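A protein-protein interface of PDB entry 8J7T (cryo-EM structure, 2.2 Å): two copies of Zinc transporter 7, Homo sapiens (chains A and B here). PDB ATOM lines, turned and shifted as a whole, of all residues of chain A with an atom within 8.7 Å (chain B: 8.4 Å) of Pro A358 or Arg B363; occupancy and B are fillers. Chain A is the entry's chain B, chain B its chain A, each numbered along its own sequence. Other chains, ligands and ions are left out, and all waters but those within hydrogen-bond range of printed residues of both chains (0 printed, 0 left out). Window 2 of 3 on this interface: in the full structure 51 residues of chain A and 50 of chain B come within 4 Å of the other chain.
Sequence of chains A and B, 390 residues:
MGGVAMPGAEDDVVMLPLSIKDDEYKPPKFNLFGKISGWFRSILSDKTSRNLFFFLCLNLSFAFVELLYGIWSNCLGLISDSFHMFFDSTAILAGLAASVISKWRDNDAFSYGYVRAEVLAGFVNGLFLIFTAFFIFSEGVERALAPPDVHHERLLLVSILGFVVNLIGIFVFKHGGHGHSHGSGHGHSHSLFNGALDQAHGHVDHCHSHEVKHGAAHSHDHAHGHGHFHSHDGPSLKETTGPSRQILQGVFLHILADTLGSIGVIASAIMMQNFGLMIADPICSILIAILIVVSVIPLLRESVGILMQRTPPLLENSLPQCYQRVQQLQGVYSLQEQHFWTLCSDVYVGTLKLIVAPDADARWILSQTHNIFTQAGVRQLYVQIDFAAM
5 positions are printed for both chains.
Leu B366 touches Ile A385 (CD2 to O, 3.5 Å).
CD2 of Leu B366 touches OD2 of Asp A386, 3.2 Å away.
Arg B363 touches Phe A387.
The backbone NH of Arg B363 lies close to the side-chain carboxylate of Asp B361, 3.4 Å away.
The backbone carbonyl oxygen (O) of Arg B363 sits at hydrogen-bond distance from the side-chain hydroxyl (OG) of Ser B367.
A ring nitrogen (ND1) of His B370 is in hydrogen-bond range of the backbone carbonyl oxygen (O) of Leu B366 (3.4 Å).
The backbone NH (N) of Val A356 lies within hydrogen-bond range of the backbone carbonyl oxygen (O) of Asp A386, 2.9 Å away.
The guanidinium group (NH2) of Arg B363 lies within hydrogen-bond range of the backbone carbonyl oxygen (O) of Pro A358 (2.9 Å).
Of the printed residues of chain B, Pro A358 touches Arg B363.
Of the printed residues of chain B, Ile A385 touches Leu B366 (3.5 Å).
Printed residues of chain B within 4 Å of Asp A386: Leu B366 (3.2 Å).
Of the printed residues of chain B, Phe A387 touches Arg B363 (3.5 Å).
Of chain A, only Pro A358 and Phe A387 come within 4 Å of Arg B363.
Printed residues of chain A within 4 Å of Leu B366: Ile A385 (3.5 Å) and Asp A386 (3.2 Å).
Phe B387 touches none of the printed residues of chain A.
The nearest printed residue of chain B that does not touch Pro A358 is Ala B362 (9.5 Å).
The nearest printed residue of chain A that does not touch Arg B363 is Ala A388 (5.0 Å).
The nearest printed residue of chain B that does not touch Phe A387 is Ala B362 (4.8 Å).
Of the 14 printed residues of chain B, 2 touch a printed residue of chain A.
Printed residues of chain B that touch a printed residue of chain A: Arg B363 and Leu B366.
Hydrophobic or aromatic side chains of chain B within 4 Å of the printed part of chain A: Leu B366.
Among the printed residues, no Asp or Glu carboxylate lies within 4 Å of a Lys or Arg side-chain nitrogen of the other chain.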
ATOM      1  N   GLY A 331      -4.103 -33.464 -28.565  1.00  0.00           N
ATOM      2  CA  GLY A 331      -4.539 -32.089 -28.503  1.00  0.00           C
ATOM      3  C   GLY A 331      -3.609 -31.086 -29.146  1.00  0.00           C
ATOM      4  O   GLY A 331      -3.929 -29.896 -29.164  1.00  0.00           O
ATOM      5  N   VAL A 332      -2.475 -31.519 -29.674  1.00  0.00           N
ATOM      6  CA  VAL A 332      -1.562 -30.635 -30.386  1.00  0.00           C
ATOM      7  C   VAL A 332      -1.998 -30.562 -31.841  1.00  0.00           C
ATOM      8  O   VAL A 332      -2.264 -31.588 -32.474  1.00  0.00           O
ATOM      9  CB  VAL A 332      -0.109 -31.125 -30.261  1.00  0.00           C
ATOM     10  CG1 VAL A 332       0.817 -30.282 -31.124  1.00  0.00           C
ATOM     11  CG2 VAL A 332       0.336 -31.113 -28.808  1.00  0.00           C
ATOM     12  N   TYR A 333      -2.107 -29.348 -32.365  1.00  0.00           N
ATOM     13  CA  TYR A 333      -2.458 -29.107 -33.755  1.00  0.00           C
ATOM     14  C   TYR A 333      -1.232 -28.844 -34.616  1.00  0.00           C
ATOM     15  O   TYR A 333      -1.099 -29.437 -35.687  1.00  0.00           O
ATOM     16  CB  TYR A 333      -3.433 -27.928 -33.849  1.00  0.00           C
ATOM     17  CG  TYR A 333      -4.824 -28.231 -33.353  1.00  0.00           C
ATOM     18  CD1 TYR A 333      -5.169 -29.504 -32.903  1.00  0.00           C
ATOM     19  CD2 TYR A 333      -5.802 -27.251 -33.349  1.00  0.00           C
ATOM     20  CE1 TYR A 333      -6.441 -29.779 -32.461  1.00  0.00           C
ATOM     21  CE2 TYR A 333      -7.076 -27.521 -32.912  1.00  0.00           C
ATOM     22  CZ  TYR A 333      -7.393 -28.779 -32.468  1.00  0.00           C
ATOM     23  OH  TYR A 333      -8.666 -29.037 -32.040  1.00  0.00           O
ATOM     24  N   ILE A 355       0.258 -24.719 -31.090  1.00  0.00           N
ATOM     25  CA  ILE A 355      -1.169 -24.500 -31.230  1.00  0.00           C
ATOM     26  C   ILE A 355      -1.841 -25.771 -30.745  1.00  0.00           C
ATOM     27  O   ILE A 355      -1.467 -26.870 -31.162  1.00  0.00           O
ATOM     28  CB  ILE A 355      -1.546 -24.182 -32.686  1.00  0.00           C
ATOM     29  CG1 ILE A 355      -1.043 -22.791 -33.062  1.00  0.00           C
ATOM     30  CG2 ILE A 355      -3.053 -24.267 -32.869  1.00  0.00           C
ATOM     31  CD1 ILE A 355      -1.428 -22.351 -34.442  1.00  0.00           C
ATOM     32  N   VAL A 356      -2.785 -25.641 -29.824  1.00  0.00           N
ATOM     33  CA  VAL A 356      -3.424 -26.807 -29.241  1.00  0.00           C
ATOM     34  C   VAL A 356      -4.928 -26.690 -29.419  1.00  0.00           C
ATOM     35  O   VAL A 356      -5.461 -25.643 -29.775  1.00  0.00           O
ATOM     36  CB  VAL A 356      -3.064 -27.011 -27.752  1.00  0.00           C
ATOM     37  CG1 VAL A 356      -1.568 -27.210 -27.591  1.00  0.00           C
ATOM     38  CG2 VAL A 356      -3.577 -25.867 -26.895  1.00  0.00           C
ATOM     39  N   ALA A 357      -5.605 -27.800 -29.158  1.00  0.00           N
ATOM     40  CA  ALA A 357      -7.050 -27.823 -29.171  1.00  0.00           C
ATOM     41  C   ALA A 357      -7.605 -26.847 -28.134  1.00  0.00           C
ATOM     42  O   ALA A 357      -6.970 -26.584 -27.113  1.00  0.00           O
ATOM     43  CB  ALA A 357      -7.548 -29.235 -28.891  1.00  0.00           C
ATOM     44  N   PRO A 358      -8.787 -26.282 -28.388  1.00  0.00           N
ATOM     45  CA  PRO A 358      -9.346 -25.293 -27.451  1.00  0.00           C
ATOM     46  C   PRO A 358      -9.587 -25.835 -26.049  1.00  0.00           C
ATOM     47  O   PRO A 358      -9.607 -25.050 -25.101  1.00  0.00           O
ATOM     48  CB  PRO A 358     -10.660 -24.872 -28.127  1.00  0.00           C
ATOM     49  CG  PRO A 358     -10.941 -25.928 -29.134  1.00  0.00           C
ATOM     50  CD  PRO A 358      -9.610 -26.411 -29.599  1.00  0.00           C
ATOM     51  N   ASP A 359      -9.750 -27.149 -25.889  1.00  0.00           N
ATOM     52  CA  ASP A 359      -9.945 -27.778 -24.586  1.00  0.00           C
ATOM     53  C   ASP A 359      -8.750 -28.633 -24.167  1.00  0.00           C
ATOM     54  O   ASP A 359      -8.876 -29.455 -23.257  1.00  0.00           O
ATOM     55  CB  ASP A 359     -11.216 -28.631 -24.604  1.00  0.00           C
ATOM     56  CG  ASP A 359     -11.128 -29.782 -25.602  1.00  0.00           C
ATOM     57  OD1 ASP A 359     -10.399 -29.644 -26.600  1.00  0.00           O
ATOM     58  OD2 ASP A 359     -11.787 -30.817 -25.400  1.00  0.00           O
ATOM     59  N   ALA A 360      -7.598 -28.465 -24.807  1.00  0.00           N
ATOM     60  CA  ALA A 360      -6.478 -29.370 -24.593  1.00  0.00           C
ATOM     61  C   ALA A 360      -5.917 -29.251 -23.176  1.00  0.00           C
ATOM     62  O   ALA A 360      -5.979 -28.195 -22.543  1.00  0.00           O
ATOM     63  CB  ALA A 360      -5.375 -29.103 -25.618  1.00  0.00           C
ATOM     64  N   ASP A 361      -5.374 -30.361 -22.683  1.00  0.00           N
ATOM     65  CA  ASP A 361      -4.727 -30.423 -21.371  1.00  0.00           C
ATOM     66  C   ASP A 361      -3.350 -29.783 -21.485  1.00  0.00           C
ATOM     67  O   ASP A 361      -2.374 -30.437 -21.849  1.00  0.00           O
ATOM     68  CB  ASP A 361      -4.655 -31.870 -20.892  1.00  0.00           C
ATOM     69  CG  ASP A 361      -4.159 -32.008 -19.459  1.00  0.00           C
ATOM     70  OD1 ASP A 361      -3.600 -31.048 -18.892  1.00  0.00           O
ATOM     71  OD2 ASP A 361      -4.339 -33.097 -18.886  1.00  0.00           O
ATOM     72  N   ALA A 362      -3.271 -28.492 -21.163  1.00  0.00           N
ATOM     73  CA  ALA A 362      -2.033 -27.749 -21.365  1.00  0.00           C
ATOM     74  C   ALA A 362      -0.965 -28.135 -20.348  1.00  0.00           C
ATOM     75  O   ALA A 362       0.225 -28.121 -20.670  1.00  0.00           O
ATOM     76  CB  ALA A 362      -2.304 -26.245 -21.315  1.00  0.00           C
ATOM     77  N   ILE A 385       1.996 -21.874 -25.309  1.00  0.00           N
ATOM     78  CA  ILE A 385       0.848 -22.681 -25.700  1.00  0.00           C
ATOM     79  C   ILE A 385      -0.294 -21.743 -26.048  1.00  0.00           C
ATOM     80  O   ILE A 385      -0.765 -20.987 -25.193  1.00  0.00           O
ATOM     81  CB  ILE A 385       0.439 -23.673 -24.598  1.00  0.00           C
ATOM     82  CG1 ILE A 385       1.568 -24.689 -24.376  1.00  0.00           C
ATOM     83  CG2 ILE A 385      -0.884 -24.346 -24.944  1.00  0.00           C
ATOM     84  CD1 ILE A 385       1.213 -25.854 -23.485  1.00  0.00           C
ATOM     85  N   ASP A 386      -0.742 -21.797 -27.294  1.00  0.00           N
ATOM     86  CA  ASP A 386      -1.866 -21.016 -27.777  1.00  0.00           C
ATOM     87  C   ASP A 386      -3.032 -21.951 -28.054  1.00  0.00           C
ATOM     88  O   ASP A 386      -2.885 -22.938 -28.778  1.00  0.00           O
ATOM     89  CB  ASP A 386      -1.484 -20.237 -29.039  1.00  0.00           C
ATOM     90  CG  ASP A 386      -0.300 -19.308 -28.816  1.00  0.00           C
ATOM     91  OD1 ASP A 386       0.858 -19.760 -28.929  1.00  0.00           O
ATOM     92  OD2 ASP A 386      -0.532 -18.114 -28.535  1.00  0.00           O
ATOM     93  N   PHE A 387      -4.181 -21.636 -27.474  1.00  0.00           N
ATOM     94  CA  PHE A 387      -5.392 -22.401 -27.720  1.00  0.00           C
ATOM     95  C   PHE A 387      -6.051 -21.912 -29.003  1.00  0.00           C
ATOM     96  O   PHE A 387      -6.336 -20.721 -29.145  1.00  0.00           O
ATOM     97  CB  PHE A 387      -6.339 -22.288 -26.526  1.00  0.00           C
ATOM     98  CG  PHE A 387      -5.820 -22.957 -25.296  1.00  0.00           C
ATOM     99  CD1 PHE A 387      -4.951 -22.298 -24.446  1.00  0.00           C
ATOM    100  CD2 PHE A 387      -6.169 -24.261 -25.006  1.00  0.00           C
ATOM    101  CE1 PHE A 387      -4.457 -22.923 -23.328  1.00  0.00           C
ATOM    102  CE2 PHE A 387      -5.674 -24.888 -23.888  1.00  0.00           C
ATOM    103  CZ  PHE A 387      -4.820 -24.221 -23.049  1.00  0.00           C
ATOM    104  N   ALA A 388      -6.271 -22.830 -29.936  1.00  0.00           N
ATOM    105  CA  ALA A 388      -6.920 -22.492 -31.192  1.00  0.00           C
ATOM    106  C   ALA A 388      -8.398 -22.196 -30.972  1.00  0.00           C
ATOM    107  O   ALA A 388      -8.994 -22.591 -29.969  1.00  0.00           O
ATOM    108  CB  ALA A 388      -6.767 -23.631 -32.198  1.00  0.00           C
ATOM    109  N   ALA A 389      -8.990 -21.474 -31.922  1.00  0.00           N
ATOM    110  CA  ALA A 389     -10.429 -21.239 -31.870  1.00  0.00           C
ATOM    111  C   ALA A 389     -11.222 -22.519 -32.113  1.00  0.00           C
ATOM    112  O   ALA A 389     -12.208 -22.779 -31.415  1.00  0.00           O
ATOM    113  CB  ALA A 389     -10.824 -20.175 -32.890  1.00  0.00           C
ATOM    114  N   MET A 390     -10.801 -23.333 -33.073  1.00  0.00           N
ATOM    115  CA  MET A 390     -11.605 -24.457 -33.534  1.00  0.00           C
ATOM    116  C   MET A 390     -10.716 -25.614 -33.980  1.00  0.00           C
ATOM    117  O   MET A 390     -10.306 -26.438 -33.166  1.00  0.00           O
ATOM    118  CB  MET A 390     -12.529 -23.989 -34.672  1.00  0.00           C
ATOM    119  CG  MET A 390     -13.911 -24.634 -34.731  1.00  0.00           C
ATOM    120  SD  MET A 390     -13.947 -26.433 -34.687  1.00  0.00           S
ATOM    121  CE  MET A 390     -12.930 -26.818 -36.112  1.00  0.00           C
ATOM    122  N   ALA B 360      -6.646 -19.653 -13.943  1.00  0.00           N
ATOM    123  CA  ALA B 360      -6.441 -18.360 -14.582  1.00  0.00           C
ATOM    124  C   ALA B 360      -6.772 -18.408 -16.074  1.00  0.00           C
ATOM    125  O   ALA B 360      -6.644 -19.443 -16.732  1.00  0.00           O
ATOM    126  CB  ALA B 360      -5.000 -17.889 -14.379  1.00  0.00           C
ATOM    127  N   ASP B 361      -7.214 -17.267 -16.597  1.00  0.00           N
ATOM    128  CA  ASP B 361      -7.517 -17.101 -18.019  1.00  0.00           C
ATOM    129  C   ASP B 361      -6.203 -16.956 -18.777  1.00  0.00           C
ATOM    130  O   ASP B 361      -5.660 -15.860 -18.901  1.00  0.00           O
ATOM    131  CB  ASP B 361      -8.437 -15.900 -18.221  1.00  0.00           C
ATOM    132  CG  ASP B 361      -8.946 -15.762 -19.649  1.00  0.00           C
ATOM    133  OD1 ASP B 361      -8.404 -16.398 -20.574  1.00  0.00           O
ATOM    134  OD2 ASP B 361      -9.913 -15.005 -19.848  1.00  0.00           O
ATOM    135  N   ALA B 362      -5.694 -18.075 -19.292  1.00  0.00           N
ATOM    136  CA  ALA B 362      -4.377 -18.074 -19.918  1.00  0.00           C
ATOM    137  C   ALA B 362      -4.391 -17.377 -21.274  1.00  0.00           C
ATOM    138  O   ALA B 362      -3.398 -16.755 -21.656  1.00  0.00           O
ATOM    139  CB  ALA B 362      -3.854 -19.503 -20.053  1.00  0.00           C
ATOM    140  N   ARG B 363      -5.492 -17.483 -22.027  1.00  0.00           N
ATOM    141  CA  ARG B 363      -5.575 -16.782 -23.309  1.00  0.00           C
ATOM    142  C   ARG B 363      -5.419 -15.282 -23.114  1.00  0.00           C
ATOM    143  O   ARG B 363      -4.617 -14.627 -23.794  1.00  0.00           O
ATOM    144  CB  ARG B 363      -6.906 -17.075 -24.004  1.00  0.00           C
ATOM    145  CG  ARG B 363      -7.185 -18.509 -24.351  1.00  0.00           C
ATOM    146  CD  ARG B 363      -8.594 -18.639 -24.907  1.00  0.00           C
ATOM    147  NE  ARG B 363      -8.919 -20.001 -25.312  1.00  0.00           N
ATOM    148  CZ  ARG B 363      -9.214 -20.987 -24.478  1.00  0.00           C
ATOM    149  NH1 ARG B 363      -9.268 -20.797 -23.171  1.00  0.00           N
ATOM    150  NH2 ARG B 363      -9.476 -22.192 -24.968  1.00  0.00           N
ATOM    151  N   TRP B 364      -6.178 -14.726 -22.172  1.00  0.00           N
ATOM    152  CA  TRP B 364      -6.118 -13.299 -21.908  1.00  0.00           C
ATOM    153  C   TRP B 364      -4.761 -12.890 -21.350  1.00  0.00           C
ATOM    154  O   TRP B 364      -4.211 -11.860 -21.750  1.00  0.00           O
ATOM    155  CB  TRP B 364      -7.248 -12.900 -20.962  1.00  0.00           C
ATOM    156  CG  TRP B 364      -7.189 -11.476 -20.590  1.00  0.00           C
ATOM    157  CD1 TRP B 364      -7.592 -10.424 -21.337  1.00  0.00           C
ATOM    158  CD2 TRP B 364      -6.655 -10.933 -19.382  1.00  0.00           C
ATOM    159  NE1 TRP B 364      -7.359  -9.253 -20.671  1.00  0.00           N
ATOM    160  CE2 TRP B 364      -6.784  -9.538 -19.465  1.00  0.00           C
ATOM    161  CE3 TRP B 364      -6.086 -11.493 -18.235  1.00  0.00           C
ATOM    162  CZ2 TRP B 364      -6.362  -8.689 -18.448  1.00  0.00           C
ATOM    163  CZ3 TRP B 364      -5.674 -10.651 -17.224  1.00  0.00           C
ATOM    164  CH2 TRP B 364      -5.811  -9.266 -17.335  1.00  0.00           C
ATOM    165  N   ILE B 365      -4.205 -13.681 -20.432  1.00  0.00           N
ATOM    166  CA  ILE B 365      -2.905 -13.355 -19.854  1.00  0.00           C
ATOM    167  C   ILE B 365      -1.830 -13.360 -20.933  1.00  0.00           C
ATOM    168  O   ILE B 365      -0.978 -12.470 -20.985  1.00  0.00           O
ATOM    169  CB  ILE B 365      -2.570 -14.324 -18.701  1.00  0.00           C
ATOM    170  CG1 ILE B 365      -3.435 -14.017 -17.474  1.00  0.00           C
ATOM    171  CG2 ILE B 365      -1.097 -14.249 -18.336  1.00  0.00           C
ATOM    172  CD1 ILE B 365      -3.246 -14.983 -16.321  1.00  0.00           C
ATOM    173  N   LEU B 366      -1.871 -14.353 -21.820  1.00  0.00           N
ATOM    174  CA  LEU B 366      -0.912 -14.427 -22.915  1.00  0.00           C
ATOM    175  C   LEU B 366      -1.019 -13.209 -23.823  1.00  0.00           C
ATOM    176  O   LEU B 366      -0.004 -12.583 -24.158  1.00  0.00           O
ATOM    177  CB  LEU B 366      -1.135 -15.716 -23.705  1.00  0.00           C
ATOM    178  CG  LEU B 366      -0.092 -16.139 -24.736  1.00  0.00           C
ATOM    179  CD1 LEU B 366       1.280 -16.257 -24.097  1.00  0.00           C
ATOM    180  CD2 LEU B 366      -0.499 -17.452 -25.376  1.00  0.00           C
ATOM    181  N   SER B 367      -2.244 -12.843 -24.217  1.00  0.00           N
ATOM    182  CA  SER B 367      -2.399 -11.698 -25.111  1.00  0.00           C
ATOM    183  C   SER B 367      -1.943 -10.407 -24.440  1.00  0.00           C
ATOM    184  O   SER B 367      -1.300  -9.563 -25.073  1.00  0.00           O
ATOM    185  CB  SER B 367      -3.843 -11.583 -25.604  1.00  0.00           C
ATOM    186  OG  SER B 367      -4.747 -11.259 -24.570  1.00  0.00           O
ATOM    187  N   GLN B 368      -2.243 -10.248 -23.151  1.00  0.00           N
ATOM    188  CA  GLN B 368      -1.823  -9.054 -22.429  1.00  0.00           C
ATOM    189  C   GLN B 368      -0.308  -8.975 -22.300  1.00  0.00           C
ATOM    190  O   GLN B 368       0.275  -7.903 -22.468  1.00  0.00           O
ATOM    191  CB  GLN B 368      -2.474  -9.028 -21.054  1.00  0.00           C
ATOM    192  CG  GLN B 368      -3.964  -8.830 -21.086  1.00  0.00           C
ATOM    193  CD  GLN B 368      -4.365  -7.443 -21.493  1.00  0.00           C
ATOM    194  OE1 GLN B 368      -5.108  -7.260 -22.451  1.00  0.00           O
ATOM    195  NE2 GLN B 368      -3.891  -6.452 -20.757  1.00  0.00           N
ATOM    196  N   THR B 369       0.343 -10.096 -21.991  1.00  0.00           N
ATOM    197  CA  THR B 369       1.794 -10.110 -21.875  1.00  0.00           C
ATOM    198  C   THR B 369       2.448  -9.772 -23.207  1.00  0.00           C
ATOM    199  O   THR B 369       3.417  -8.999 -23.261  1.00  0.00           O
ATOM    200  CB  THR B 369       2.261 -11.479 -21.376  1.00  0.00           C
ATOM    201  OG1 THR B 369       1.604 -11.790 -20.145  1.00  0.00           O
ATOM    202  CG2 THR B 369       3.758 -11.500 -21.172  1.00  0.00           C
ATOM    203  N   HIS B 370       1.909 -10.316 -24.295  1.00  0.00           N
ATOM    204  CA  HIS B 370       2.434  -9.981 -25.609  1.00  0.00           C
ATOM    205  C   HIS B 370       2.235  -8.508 -25.927  1.00  0.00           C
ATOM    206  O   HIS B 370       3.127  -7.870 -26.487  1.00  0.00           O
ATOM    207  CB  HIS B 370       1.803 -10.875 -26.669  1.00  0.00           C
ATOM    208  CG  HIS B 370       2.634 -12.074 -26.987  1.00  0.00           C
ATOM    209  ND1 HIS B 370       2.431 -13.297 -26.390  1.00  0.00           N
ATOM    210  CD2 HIS B 370       3.686 -12.232 -27.822  1.00  0.00           C
ATOM    211  CE1 HIS B 370       3.323 -14.158 -26.843  1.00  0.00           C
ATOM    212  NE2 HIS B 370       4.092 -13.540 -27.717  1.00  0.00           N
ATOM    213  N   ASN B 371       1.085  -7.943 -25.561  1.00  0.00           N
ATOM    214  CA  ASN B 371       0.860  -6.520 -25.797  1.00  0.00           C
ATOM    215  C   ASN B 371       1.848  -5.671 -25.009  1.00  0.00           C
ATOM    216  O   ASN B 371       2.419  -4.708 -25.537  1.00  0.00           O
ATOM    217  CB  ASN B 371      -0.570  -6.149 -25.414  1.00  0.00           C
ATOM    218  CG  ASN B 371      -1.591  -6.683 -26.389  1.00  0.00           C
ATOM    219  OD1 ASN B 371      -2.767  -6.823 -26.058  1.00  0.00           O
ATOM    220  ND2 ASN B 371      -1.149  -6.993 -27.597  1.00  0.00           N
ATOM    221  N   ILE B 385       3.388 -20.520 -19.800  1.00  0.00           N
ATOM    222  CA  ILE B 385       2.425 -20.331 -18.725  1.00  0.00           C
ATOM    223  C   ILE B 385       2.294 -21.641 -17.968  1.00  0.00           C
ATOM    224  O   ILE B 385       1.878 -22.654 -18.540  1.00  0.00           O
ATOM    225  CB  ILE B 385       1.061 -19.851 -19.252  1.00  0.00           C
ATOM    226  CG1 ILE B 385       1.212 -18.462 -19.884  1.00  0.00           C
ATOM    227  CG2 ILE B 385       0.018 -19.870 -18.140  1.00  0.00           C
ATOM    228  CD1 ILE B 385      -0.084 -17.775 -20.238  1.00  0.00           C
ATOM    229  N   PHE B 387       0.474 -23.417 -14.701  1.00  0.00           N
ATOM    230  CA  PHE B 387      -0.592 -23.317 -13.717  1.00  0.00           C
ATOM    231  C   PHE B 387      -0.103 -23.859 -12.380  1.00  0.00           C
ATOM    232  O   PHE B 387       0.362 -24.998 -12.300  1.00  0.00           O
ATOM    233  CB  PHE B 387      -1.832 -24.063 -14.205  1.00  0.00           C
ATOM    234  CG  PHE B 387      -2.475 -23.427 -15.393  1.00  0.00           C
ATOM    235  CD1 PHE B 387      -2.025 -23.698 -16.671  1.00  0.00           C
ATOM    236  CD2 PHE B 387      -3.509 -22.525 -15.232  1.00  0.00           C
ATOM    237  CE1 PHE B 387      -2.601 -23.095 -17.760  1.00  0.00           C
ATOM    238  CE2 PHE B 387      -4.086 -21.920 -16.322  1.00  0.00           C
ATOM    239  CZ  PHE B 387      -3.635 -22.203 -17.584  1.00  0.00           C
